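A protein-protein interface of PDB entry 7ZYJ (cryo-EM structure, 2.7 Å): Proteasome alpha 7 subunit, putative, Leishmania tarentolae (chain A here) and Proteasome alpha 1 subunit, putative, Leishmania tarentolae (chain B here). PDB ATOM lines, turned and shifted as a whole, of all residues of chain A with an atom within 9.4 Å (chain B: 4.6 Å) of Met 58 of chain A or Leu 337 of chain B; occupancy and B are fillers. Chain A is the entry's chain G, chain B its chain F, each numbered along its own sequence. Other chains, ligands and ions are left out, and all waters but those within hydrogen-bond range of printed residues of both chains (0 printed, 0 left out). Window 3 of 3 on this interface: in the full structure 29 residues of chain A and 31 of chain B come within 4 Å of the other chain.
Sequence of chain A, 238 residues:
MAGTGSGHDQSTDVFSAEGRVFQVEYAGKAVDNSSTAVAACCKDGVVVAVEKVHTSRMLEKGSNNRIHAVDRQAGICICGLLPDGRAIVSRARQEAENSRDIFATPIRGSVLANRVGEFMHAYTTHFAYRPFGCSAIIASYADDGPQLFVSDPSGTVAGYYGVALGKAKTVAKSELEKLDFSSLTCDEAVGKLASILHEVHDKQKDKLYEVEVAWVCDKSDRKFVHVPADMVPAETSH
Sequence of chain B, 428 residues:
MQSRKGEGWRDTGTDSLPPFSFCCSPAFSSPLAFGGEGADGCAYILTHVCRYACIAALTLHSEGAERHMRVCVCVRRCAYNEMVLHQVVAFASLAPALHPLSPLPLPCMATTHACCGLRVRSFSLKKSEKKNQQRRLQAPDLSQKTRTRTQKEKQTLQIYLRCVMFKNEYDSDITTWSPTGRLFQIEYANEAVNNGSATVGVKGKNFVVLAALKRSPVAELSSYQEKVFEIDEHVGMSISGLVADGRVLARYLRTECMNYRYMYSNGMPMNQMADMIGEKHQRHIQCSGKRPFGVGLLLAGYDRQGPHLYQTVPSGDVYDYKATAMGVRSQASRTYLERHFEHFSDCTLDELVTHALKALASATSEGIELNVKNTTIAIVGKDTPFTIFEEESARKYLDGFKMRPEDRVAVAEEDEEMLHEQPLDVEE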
ATOM      1  N   HIS A  54      -5.702  25.658  12.337  1.00  0.00           N
ATOM      2  CA  HIS A  54      -6.352  24.448  11.862  1.00  0.00           C
ATOM      3  C   HIS A  54      -7.093  24.721  10.561  1.00  0.00           C
ATOM      4  O   HIS A  54      -7.809  25.718  10.433  1.00  0.00           O
ATOM      5  CB  HIS A  54      -7.321  23.916  12.916  1.00  0.00           C
ATOM      6  CG  HIS A  54      -6.656  23.484  14.184  1.00  0.00           C
ATOM      7  ND1 HIS A  54      -5.456  22.805  14.201  1.00  0.00           N
ATOM      8  CD2 HIS A  54      -7.020  23.636  15.480  1.00  0.00           C
ATOM      9  CE1 HIS A  54      -5.112  22.555  15.452  1.00  0.00           C
ATOM     10  NE2 HIS A  54      -6.044  23.048  16.247  1.00  0.00           N
ATOM     11  N   THR A  55      -6.912  23.831   9.591  1.00  0.00           N
ATOM     12  CA  THR A  55      -7.633  23.910   8.329  1.00  0.00           C
ATOM     13  C   THR A  55      -8.953  23.154   8.366  1.00  0.00           C
ATOM     14  O   THR A  55      -9.669  23.136   7.360  1.00  0.00           O
ATOM     15  CB  THR A  55      -6.765  23.376   7.186  1.00  0.00           C
ATOM     16  OG1 THR A  55      -6.615  21.957   7.319  1.00  0.00           O
ATOM     17  CG2 THR A  55      -5.393  24.031   7.208  1.00  0.00           C
ATOM     18  N   SER A  56      -9.287  22.536   9.495  1.00  0.00           N
ATOM     19  CA  SER A  56     -10.548  21.830   9.651  1.00  0.00           C
ATOM     20  C   SER A  56     -11.080  22.074  11.053  1.00  0.00           C
ATOM     21  O   SER A  56     -10.314  22.203  12.012  1.00  0.00           O
ATOM     22  CB  SER A  56     -10.389  20.326   9.400  1.00  0.00           C
ATOM     23  OG  SER A  56     -11.585  19.631   9.702  1.00  0.00           O
ATOM     24  N   ARG A  57     -12.403  22.135  11.164  1.00  0.00           N
ATOM     25  CA  ARG A  57     -13.071  22.288  12.448  1.00  0.00           C
ATOM     26  C   ARG A  57     -13.368  20.953  13.117  1.00  0.00           C
ATOM     27  O   ARG A  57     -13.863  20.939  14.248  1.00  0.00           O
ATOM     28  CB  ARG A  57     -14.372  23.078  12.274  1.00  0.00           C
ATOM     29  CG  ARG A  57     -15.402  22.383  11.400  1.00  0.00           C
ATOM     30  CD  ARG A  57     -16.657  23.226  11.248  1.00  0.00           C
ATOM     31  NE  ARG A  57     -17.381  23.354  12.508  1.00  0.00           N
ATOM     32  CZ  ARG A  57     -18.338  24.242  12.735  1.00  0.00           C
ATOM     33  NH1 ARG A  57     -18.719  25.101  11.802  1.00  0.00           N
ATOM     34  NH2 ARG A  57     -18.929  24.269  13.925  1.00  0.00           N
ATOM     35  N   MET A  58     -13.076  19.837  12.449  1.00  0.00           N
ATOM     36  CA  MET A  58     -13.347  18.505  12.971  1.00  0.00           C
ATOM     37  C   MET A  58     -12.110  17.855  13.579  1.00  0.00           C
ATOM     38  O   MET A  58     -12.128  16.655  13.870  1.00  0.00           O
ATOM     39  CB  MET A  58     -13.920  17.619  11.867  1.00  0.00           C
ATOM     40  CG  MET A  58     -15.020  18.279  11.054  1.00  0.00           C
ATOM     41  SD  MET A  58     -16.040  17.087  10.173  1.00  0.00           S
ATOM     42  CE  MET A  58     -15.168  16.998   8.612  1.00  0.00           C
ATOM     43  N   LEU A  59     -11.038  18.617  13.769  1.00  0.00           N
ATOM     44  CA  LEU A  59      -9.823  18.077  14.356  1.00  0.00           C
ATOM     45  C   LEU A  59     -10.013  17.808  15.843  1.00  0.00           C
ATOM     46  O   LEU A  59     -10.623  18.597  16.569  1.00  0.00           O
ATOM     47  CB  LEU A  59      -8.653  19.038  14.150  1.00  0.00           C
ATOM     48  CG  LEU A  59      -7.998  19.025  12.769  1.00  0.00           C
ATOM     49  CD1 LEU A  59      -7.070  20.215  12.606  1.00  0.00           C
ATOM     50  CD2 LEU A  59      -7.242  17.727  12.557  1.00  0.00           C
ATOM     51  N   GLU A  60      -9.482  16.674  16.290  1.00  0.00           N
ATOM     52  CA  GLU A  60      -9.491  16.348  17.707  1.00  0.00           C
ATOM     53  C   GLU A  60      -8.565  17.297  18.462  1.00  0.00           C
ATOM     54  O   GLU A  60      -7.545  17.750  17.939  1.00  0.00           O
ATOM     55  CB  GLU A  60      -9.058  14.897  17.919  1.00  0.00           C
ATOM     56  CG  GLU A  60      -9.069  14.420  19.363  1.00  0.00           C
ATOM     57  CD  GLU A  60     -10.463  14.388  19.961  1.00  0.00           C
ATOM     58  OE1 GLU A  60     -11.440  14.251  19.195  1.00  0.00           O
ATOM     59  OE2 GLU A  60     -10.583  14.499  21.199  1.00  0.00           O
ATOM     60  N   LYS A  61      -8.940  17.610  19.700  1.00  0.00           N
ATOM     61  CA  LYS A  61      -8.154  18.539  20.503  1.00  0.00           C
ATOM     62  C   LYS A  61      -6.766  17.966  20.766  1.00  0.00           C
ATOM     63  O   LYS A  61      -6.622  16.793  21.120  1.00  0.00           O
ATOM     64  CB  LYS A  61      -8.865  18.836  21.821  1.00  0.00           C
ATOM     65  CG  LYS A  61      -8.135  19.834  22.703  1.00  0.00           C
ATOM     66  CD  LYS A  61      -8.045  21.193  22.028  1.00  0.00           C
ATOM     67  CE  LYS A  61      -9.409  21.860  21.947  1.00  0.00           C
ATOM     68  NZ  LYS A  61      -9.329  23.220  21.345  1.00  0.00           N
ATOM     69  N   SER A  63      -4.444  17.944  18.318  1.00  0.00           N
ATOM     70  CA  SER A  63      -3.885  17.530  17.041  1.00  0.00           C
ATOM     71  C   SER A  63      -2.771  18.474  16.606  1.00  0.00           C
ATOM     72  O   SER A  63      -2.807  19.679  16.867  1.00  0.00           O
ATOM     73  CB  SER A  63      -4.974  17.486  15.969  1.00  0.00           C
ATOM     74  OG  SER A  63      -4.419  17.241  14.689  1.00  0.00           O
ATOM     75  N   ASN A  64      -1.771  17.903  15.933  1.00  0.00           N
ATOM     76  CA  ASN A  64      -0.634  18.659  15.407  1.00  0.00           C
ATOM     77  C   ASN A  64       0.102  19.398  16.520  1.00  0.00           C
ATOM     78  O   ASN A  64       0.341  20.605  16.437  1.00  0.00           O
ATOM     79  CB  ASN A  64      -1.075  19.629  14.311  1.00  0.00           C
ATOM     80  CG  ASN A  64      -1.682  18.922  13.120  1.00  0.00           C
ATOM     81  OD1 ASN A  64      -1.069  18.030  12.533  1.00  0.00           O
ATOM     82  ND2 ASN A  64      -2.899  19.310  12.762  1.00  0.00           N
ATOM     83  N   LEU A 208      -9.653  29.077  12.323  1.00  0.00           N
ATOM     84  CA  LEU A 208      -9.507  28.105  13.402  1.00  0.00           C
ATOM     85  C   LEU A 208      -8.100  28.227  13.973  1.00  0.00           C
ATOM     86  O   LEU A 208      -7.119  27.888  13.302  1.00  0.00           O
ATOM     87  CB  LEU A 208      -9.781  26.687  12.905  1.00  0.00           C
ATOM     88  CG  LEU A 208     -11.226  26.181  12.976  1.00  0.00           C
ATOM     89  CD1 LEU A 208     -11.697  26.105  14.422  1.00  0.00           C
ATOM     90  CD2 LEU A 208     -12.170  27.041  12.146  1.00  0.00           C
ATOM     91  N   VAL B 200     -13.958   7.906   3.852  1.00  0.00           N
ATOM     92  CA  VAL B 200     -14.482   8.718   4.944  1.00  0.00           C
ATOM     93  C   VAL B 200     -14.206   8.001   6.258  1.00  0.00           C
ATOM     94  O   VAL B 200     -14.405   6.787   6.360  1.00  0.00           O
ATOM     95  CB  VAL B 200     -15.993   8.979   4.776  1.00  0.00           C
ATOM     96  CG1 VAL B 200     -16.617   9.433   6.087  1.00  0.00           C
ATOM     97  CG2 VAL B 200     -16.240   9.999   3.678  1.00  0.00           C
ATOM     98  N   GLY B 201     -13.742   8.741   7.254  1.00  0.00           N
ATOM     99  CA  GLY B 201     -13.546   8.207   8.593  1.00  0.00           C
ATOM    100  C   GLY B 201     -14.379   8.978   9.597  1.00  0.00           C
ATOM    101  O   GLY B 201     -14.424  10.210   9.558  1.00  0.00           O
ATOM    102  N   VAL B 202     -15.041   8.246  10.491  1.00  0.00           N
ATOM    103  CA  VAL B 202     -15.909   8.828  11.507  1.00  0.00           C
ATOM    104  C   VAL B 202     -15.569   8.203  12.852  1.00  0.00           C
ATOM    105  O   VAL B 202     -15.427   6.980  12.959  1.00  0.00           O
ATOM    106  CB  VAL B 202     -17.399   8.616  11.166  1.00  0.00           C
ATOM    107  CG1 VAL B 202     -18.275   9.040  12.322  1.00  0.00           C
ATOM    108  CG2 VAL B 202     -17.772   9.384   9.908  1.00  0.00           C
ATOM    109  N   TYR B 321      -8.397  13.385  14.116  1.00  0.00           N
ATOM    110  CA  TYR B 321      -9.669  13.849  13.586  1.00  0.00           C
ATOM    111  C   TYR B 321     -10.838  13.237  14.343  1.00  0.00           C
ATOM    112  O   TYR B 321     -10.814  12.062  14.718  1.00  0.00           O
ATOM    113  CB  TYR B 321      -9.804  13.500  12.099  1.00  0.00           C
ATOM    114  CG  TYR B 321      -9.403  14.607  11.154  1.00  0.00           C
ATOM    115  CD1 TYR B 321     -10.132  15.786  11.086  1.00  0.00           C
ATOM    116  CD2 TYR B 321      -8.304  14.467  10.318  1.00  0.00           C
ATOM    117  CE1 TYR B 321      -9.773  16.797  10.218  1.00  0.00           C
ATOM    118  CE2 TYR B 321      -7.939  15.473   9.447  1.00  0.00           C
ATOM    119  CZ  TYR B 321      -8.675  16.635   9.401  1.00  0.00           C
ATOM    120  OH  TYR B 321      -8.309  17.638   8.535  1.00  0.00           O
ATOM    121  N   LYS B 322     -11.869  14.056  14.564  1.00  0.00           N
ATOM    122  CA  LYS B 322     -13.165  13.527  14.971  1.00  0.00           C
ATOM    123  C   LYS B 322     -13.869  12.862  13.795  1.00  0.00           C
ATOM    124  O   LYS B 322     -14.493  11.808  13.952  1.00  0.00           O
ATOM    125  CB  LYS B 322     -14.036  14.642  15.548  1.00  0.00           C
ATOM    126  CG  LYS B 322     -13.605  15.142  16.914  1.00  0.00           C
ATOM    127  CD  LYS B 322     -14.605  16.146  17.461  1.00  0.00           C
ATOM    128  CE  LYS B 322     -14.393  16.392  18.945  1.00  0.00           C
ATOM    129  NZ  LYS B 322     -13.312  17.383  19.195  1.00  0.00           N
ATOM    130  N   ALA B 323     -13.777  13.472  12.616  1.00  0.00           N
ATOM    131  CA  ALA B 323     -14.319  12.920  11.385  1.00  0.00           C
ATOM    132  C   ALA B 323     -13.648  13.635  10.224  1.00  0.00           C
ATOM    133  O   ALA B 323     -13.379  14.836  10.306  1.00  0.00           O
ATOM    134  CB  ALA B 323     -15.840  13.083  11.310  1.00  0.00           C
ATOM    135  N   THR B 324     -13.377  12.899   9.152  1.00  0.00           N
ATOM    136  CA  THR B 324     -12.654  13.467   8.021  1.00  0.00           C
ATOM    137  C   THR B 324     -12.937  12.637   6.776  1.00  0.00           C
ATOM    138  O   THR B 324     -13.594  11.594   6.831  1.00  0.00           O
ATOM    139  CB  THR B 324     -11.152  13.538   8.306  1.00  0.00           C
ATOM    140  OG1 THR B 324     -10.483  14.166   7.205  1.00  0.00           O
ATOM    141  CG2 THR B 324     -10.582  12.146   8.511  1.00  0.00           C
ATOM    142  N   ALA B 325     -12.431  13.118   5.644  1.00  0.00           N
ATOM    143  CA  ALA B 325     -12.568  12.426   4.372  1.00  0.00           C
ATOM    144  C   ALA B 325     -11.389  12.801   3.489  1.00  0.00           C
ATOM    145  O   ALA B 325     -10.750  13.835   3.694  1.00  0.00           O
ATOM    146  CB  ALA B 325     -13.889  12.776   3.680  1.00  0.00           C
ATOM    147  N   SER B 333     -18.016  15.437   1.089  1.00  0.00           N
ATOM    148  CA  SER B 333     -18.074  14.601   2.283  1.00  0.00           C
ATOM    149  C   SER B 333     -17.650  15.382   3.520  1.00  0.00           C
ATOM    150  O   SER B 333     -18.278  15.272   4.579  1.00  0.00           O
ATOM    151  CB  SER B 333     -17.192  13.367   2.103  1.00  0.00           C
ATOM    152  OG  SER B 333     -17.686  12.537   1.066  1.00  0.00           O
ATOM    153  N   ARG B 334     -16.586  16.179   3.403  1.00  0.00           N
ATOM    154  CA  ARG B 334     -16.120  16.960   4.544  1.00  0.00           C
ATOM    155  C   ARG B 334     -17.147  18.006   4.964  1.00  0.00           C
ATOM    156  O   ARG B 334     -17.389  18.197   6.161  1.00  0.00           O
ATOM    157  CB  ARG B 334     -14.779  17.618   4.221  1.00  0.00           C
ATOM    158  CG  ARG B 334     -13.615  16.643   4.165  1.00  0.00           C
ATOM    159  CD  ARG B 334     -12.280  17.367   4.200  1.00  0.00           C
ATOM    160  NE  ARG B 334     -12.067  18.185   3.012  1.00  0.00           N
ATOM    161  CZ  ARG B 334     -11.525  17.742   1.886  1.00  0.00           C
ATOM    162  NH1 ARG B 334     -11.128  16.486   1.757  1.00  0.00           N
ATOM    163  NH2 ARG B 334     -11.376  18.580   0.864  1.00  0.00           N
ATOM    164  N   THR B 335     -17.770  18.688   3.999  1.00  0.00           N
ATOM    165  CA  THR B 335     -18.727  19.733   4.353  1.00  0.00           C
ATOM    166  C   THR B 335     -20.022  19.135   4.887  1.00  0.00           C
ATOM    167  O   THR B 335     -20.738  19.782   5.661  1.00  0.00           O
ATOM    168  CB  THR B 335     -18.997  20.650   3.157  1.00  0.00           C
ATOM    169  OG1 THR B 335     -19.752  21.789   3.592  1.00  0.00           O
ATOM    170  CG2 THR B 335     -19.780  19.933   2.078  1.00  0.00           C
ATOM    171  N   TYR B 336     -20.346  17.900   4.490  1.00  0.00           N
ATOM    172  CA  TYR B 336     -21.463  17.209   5.124  1.00  0.00           C
ATOM    173  C   TYR B 336     -21.117  16.819   6.555  1.00  0.00           C
ATOM    174  O   TYR B 336     -21.920  17.016   7.474  1.00  0.00           O
ATOM    175  CB  TYR B 336     -21.860  15.973   4.315  1.00  0.00           C
ATOM    176  CG  TYR B 336     -22.660  14.969   5.118  1.00  0.00           C
ATOM    177  CD1 TYR B 336     -24.032  15.112   5.276  1.00  0.00           C
ATOM    178  CD2 TYR B 336     -22.043  13.878   5.720  1.00  0.00           C
ATOM    179  CE1 TYR B 336     -24.765  14.201   6.012  1.00  0.00           C
ATOM    180  CE2 TYR B 336     -22.768  12.964   6.458  1.00  0.00           C
ATOM    181  CZ  TYR B 336     -24.128  13.130   6.600  1.00  0.00           C
ATOM    182  OH  TYR B 336     -24.853  12.220   7.333  1.00  0.00           O
ATOM    183  N   LEU B 337     -19.922  16.257   6.760  1.00  0.00           N
ATOM    184  CA  LEU B 337     -19.518  15.832   8.096  1.00  0.00           C
ATOM    185  C   LEU B 337     -19.399  17.012   9.048  1.00  0.00           C
ATOM    186  O   LEU B 337     -19.607  16.857  10.257  1.00  0.00           O
ATOM    187  CB  LEU B 337     -18.194  15.070   8.026  1.00  0.00           C
ATOM    188  CG  LEU B 337     -18.247  13.633   7.505  1.00  0.00           C
ATOM    189  CD1 LEU B 337     -16.855  13.149   7.131  1.00  0.00           C
ATOM    190  CD2 LEU B 337     -18.883  12.708   8.532  1.00  0.00           C
ATOM    191  N   GLU B 338     -19.077  18.196   8.528  1.00  0.00           N
ATOM    192  CA  GLU B 338     -18.979  19.393   9.364  1.00  0.00           C
ATOM    193  C   GLU B 338     -20.322  19.854   9.913  1.00  0.00           C
ATOM    194  O   GLU B 338     -20.363  20.889  10.591  1.00  0.00           O
ATOM    195  CB  GLU B 338     -18.327  20.531   8.578  1.00  0.00           C
ATOM    196  CG  GLU B 338     -16.831  20.373   8.383  1.00  0.00           C
ATOM    197  CD  GLU B 338     -16.250  21.436   7.472  1.00  0.00           C
ATOM    198  OE1 GLU B 338     -17.036  22.175   6.845  1.00  0.00           O
ATOM    199  OE2 GLU B 338     -15.009  21.528   7.383  1.00  0.00           O
ATOM    200  N   ARG B 339     -21.412  19.135   9.646  1.00  0.00           N
ATOM    201  CA  ARG B 339     -22.721  19.464  10.189  1.00  0.00           C
ATOM    202  C   ARG B 339     -23.211  18.477  11.236  1.00  0.00           C
ATOM    203  O   ARG B 339     -24.093  18.821  12.023  1.00  0.00           O
ATOM    204  CB  ARG B 339     -23.762  19.540   9.064  1.00  0.00           C
ATOM    205  CG  ARG B 339     -23.578  20.714   8.118  1.00  0.00           C
ATOM    206  CD  ARG B 339     -24.696  20.767   7.090  1.00  0.00           C
ATOM    207  NE  ARG B 339     -24.602  19.683   6.121  1.00  0.00           N
ATOM    208  CZ  ARG B 339     -24.619  19.850   4.805  1.00  0.00           C
ATOM    209  NH1 ARG B 339     -24.725  21.051   4.262  1.00  0.00           N
ATOM    210  NH2 ARG B 339     -24.528  18.784   4.015  1.00  0.00           N
ATOM    211  N   HIS B 340     -22.660  17.262  11.264  1.00  0.00           N
ATOM    212  CA  HIS B 340     -23.113  16.223  12.179  1.00  0.00           C
ATOM    213  C   HIS B 340     -21.995  15.680  13.061  1.00  0.00           C
ATOM    214  O   HIS B 340     -22.237  14.753  13.843  1.00  0.00           O
ATOM    215  CB  HIS B 340     -23.754  15.070  11.400  1.00  0.00           C
ATOM    216  CG  HIS B 340     -24.888  15.490  10.518  1.00  0.00           C
ATOM    217  ND1 HIS B 340     -24.708  16.254   9.386  1.00  0.00           N
ATOM    218  CD2 HIS B 340     -26.218  15.247  10.599  1.00  0.00           C
ATOM    219  CE1 HIS B 340     -25.877  16.467   8.809  1.00  0.00           C
ATOM    220  NE2 HIS B 340     -26.810  15.866   9.526  1.00  0.00           N
ATOM    221  N   PHE B 341     -20.781  16.225  12.961  1.00  0.00           N
ATOM    222  CA  PHE B 341     -19.655  15.656  13.691  1.00  0.00           C
ATOM    223  C   PHE B 341     -19.738  15.891  15.194  1.00  0.00           C
ATOM    224  O   PHE B 341     -19.372  14.995  15.965  1.00  0.00           O
ATOM    225  CB  PHE B 341     -18.334  16.205  13.139  1.00  0.00           C
ATOM    226  CG  PHE B 341     -17.972  17.570  13.649  1.00  0.00           C
ATOM    227  CD1 PHE B 341     -18.576  18.700  13.128  1.00  0.00           C
ATOM    228  CD2 PHE B 341     -17.014  17.722  14.636  1.00  0.00           C
ATOM    229  CE1 PHE B 341     -18.241  19.958  13.590  1.00  0.00           C
ATOM    230  CE2 PHE B 341     -16.675  18.977  15.103  1.00  0.00           C
ATOM    231  CZ  PHE B 341     -17.289  20.096  14.579  1.00  0.00           C
ATOM    232  N   PHE B 344     -21.348  13.109  17.017  1.00  0.00           N
ATOM    233  CA  PHE B 344     -20.828  11.753  16.874  1.00  0.00           C
ATOM    234  C   PHE B 344     -20.502  11.110  18.215  1.00  0.00           C
ATOM    235  O   PHE B 344     -20.484   9.879  18.310  1.00  0.00           O
ATOM    236  CB  PHE B 344     -19.585  11.751  15.984  1.00  0.00           C
ATOM    237  CG  PHE B 344     -19.888  11.929  14.525  1.00  0.00           C
ATOM    238  CD1 PHE B 344     -21.171  11.733  14.043  1.00  0.00           C
ATOM    239  CD2 PHE B 344     -18.891  12.283  13.635  1.00  0.00           C
ATOM    240  CE1 PHE B 344     -21.455  11.895  12.703  1.00  0.00           C
ATOM    241  CE2 PHE B 344     -19.170  12.448  12.292  1.00  0.00           C
ATOM    242  CZ  PHE B 344     -20.454  12.254  11.826  1.00  0.00           C
ATOM    243  N   ALA B 359     -21.810  10.446   4.191  1.00  0.00           N
ATOM    244  CA  ALA B 359     -20.635  11.207   3.784  1.00  0.00           C
ATOM    245  C   ALA B 359     -19.997  10.614   2.534  1.00  0.00           C
ATOM    246  O   ALA B 359     -19.608  11.349   1.619  1.00  0.00           O
ATOM    247  CB  ALA B 359     -19.626  11.266   4.929  1.00  0.00           C
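OE1 of Glu 60 of chain A is in salt-bridge range of NZ of Lys 322 of chain B, at 3.6 Å. The side-chain sulfur (SD) of Met 58 of chain A lies close to the backbone carbonyl oxygen (O) of Leu 337 of chain B (3.6 Å). O of Ala 323 of chain B lies close to SD of Met 58 of chain A (3.5 Å). The backbone carbonyl oxygen (O) of Met 58 of chain A is in hydrogen-bond range of the backbone NH (N) of Lys 322 of chain B (2.7 Å). SD of Met 58 of chain A sits at hydrogen-bond distance from N of Glu 338 of chain B.
The guanidinium group of Arg 334 of chain B is in hydrogen-bond range of the backbone carbonyl oxygen of Ala 325 of chain B, at 3.3 Å. The backbone NH (N) of Met 58 of chain A is in hydrogen-bond range of the side-chain hydroxyl (OG) of Ser 56 of chain A (3.1 Å).
Tyr 321 of chain B touches Ser 56 of chain A (CE1 to OG, 3.4 Å). Glu 338 of chain B touches Arg 57 of chain A. O of Arg 57 of chain A touches CE2 of Phe 341 of chain B, 3.5 Å away. O of Met 58 of chain A touches CD1 of Tyr 321 of chain B, 3.5 Å away. Met 58 of chain A touches Arg 334 of chain B. Phe 341 of chain B touches Met 58 of chain A (CB to SD, 3.9 Å). Leu 59 of chain A touches Tyr 321 of chain B. NZ of Lys 322 of chain B touches O of Leu 59 of chain A, at 3.9 Å. Glu 60 of chain A touches Tyr 321 of chain B.
Of chain A, only Met 58 comes within 4 Å of Leu 337 of chain B. Printed residues of chain B within 4 Å of Ser 56 of chain A: Tyr 321 (3.4 Å). Of the printed residues of chain B, Leu 59 of chain A touches Tyr 321 (3.6 Å) and Lys 322 (3.9 Å). Of the printed residues of chain B, Arg 57 of chain A touches Glu 338 and Phe 341. Printed residues of chain B within 4 Å of Glu 60 of chain A: Tyr 321 and Lys 322. Leu 208 of chain A touches none of the printed residues of chain B. Asn 64 of chain A touches none of the printed residues of chain B. The nearest residue of chain A that does not touch Leu 337 of chain B is Arg 57 of chain A (7.0 Å).
Printed residues of chain B that touch a printed residue of chain A: Tyr 321, Lys 322, Ala 323, Arg 334, Leu 337, Glu 338 and Phe 341. Hydrophobic or aromatic side chains of chain B that line the printed part of chain A: Tyr 321, Leu 337 and Phe 341. Among the printed residues, Asp or Glu carboxylates within 4 Å of a Lys or Arg side-chain nitrogen of the other chain: Glu 60 of chain A with Lys 322 of chain B.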
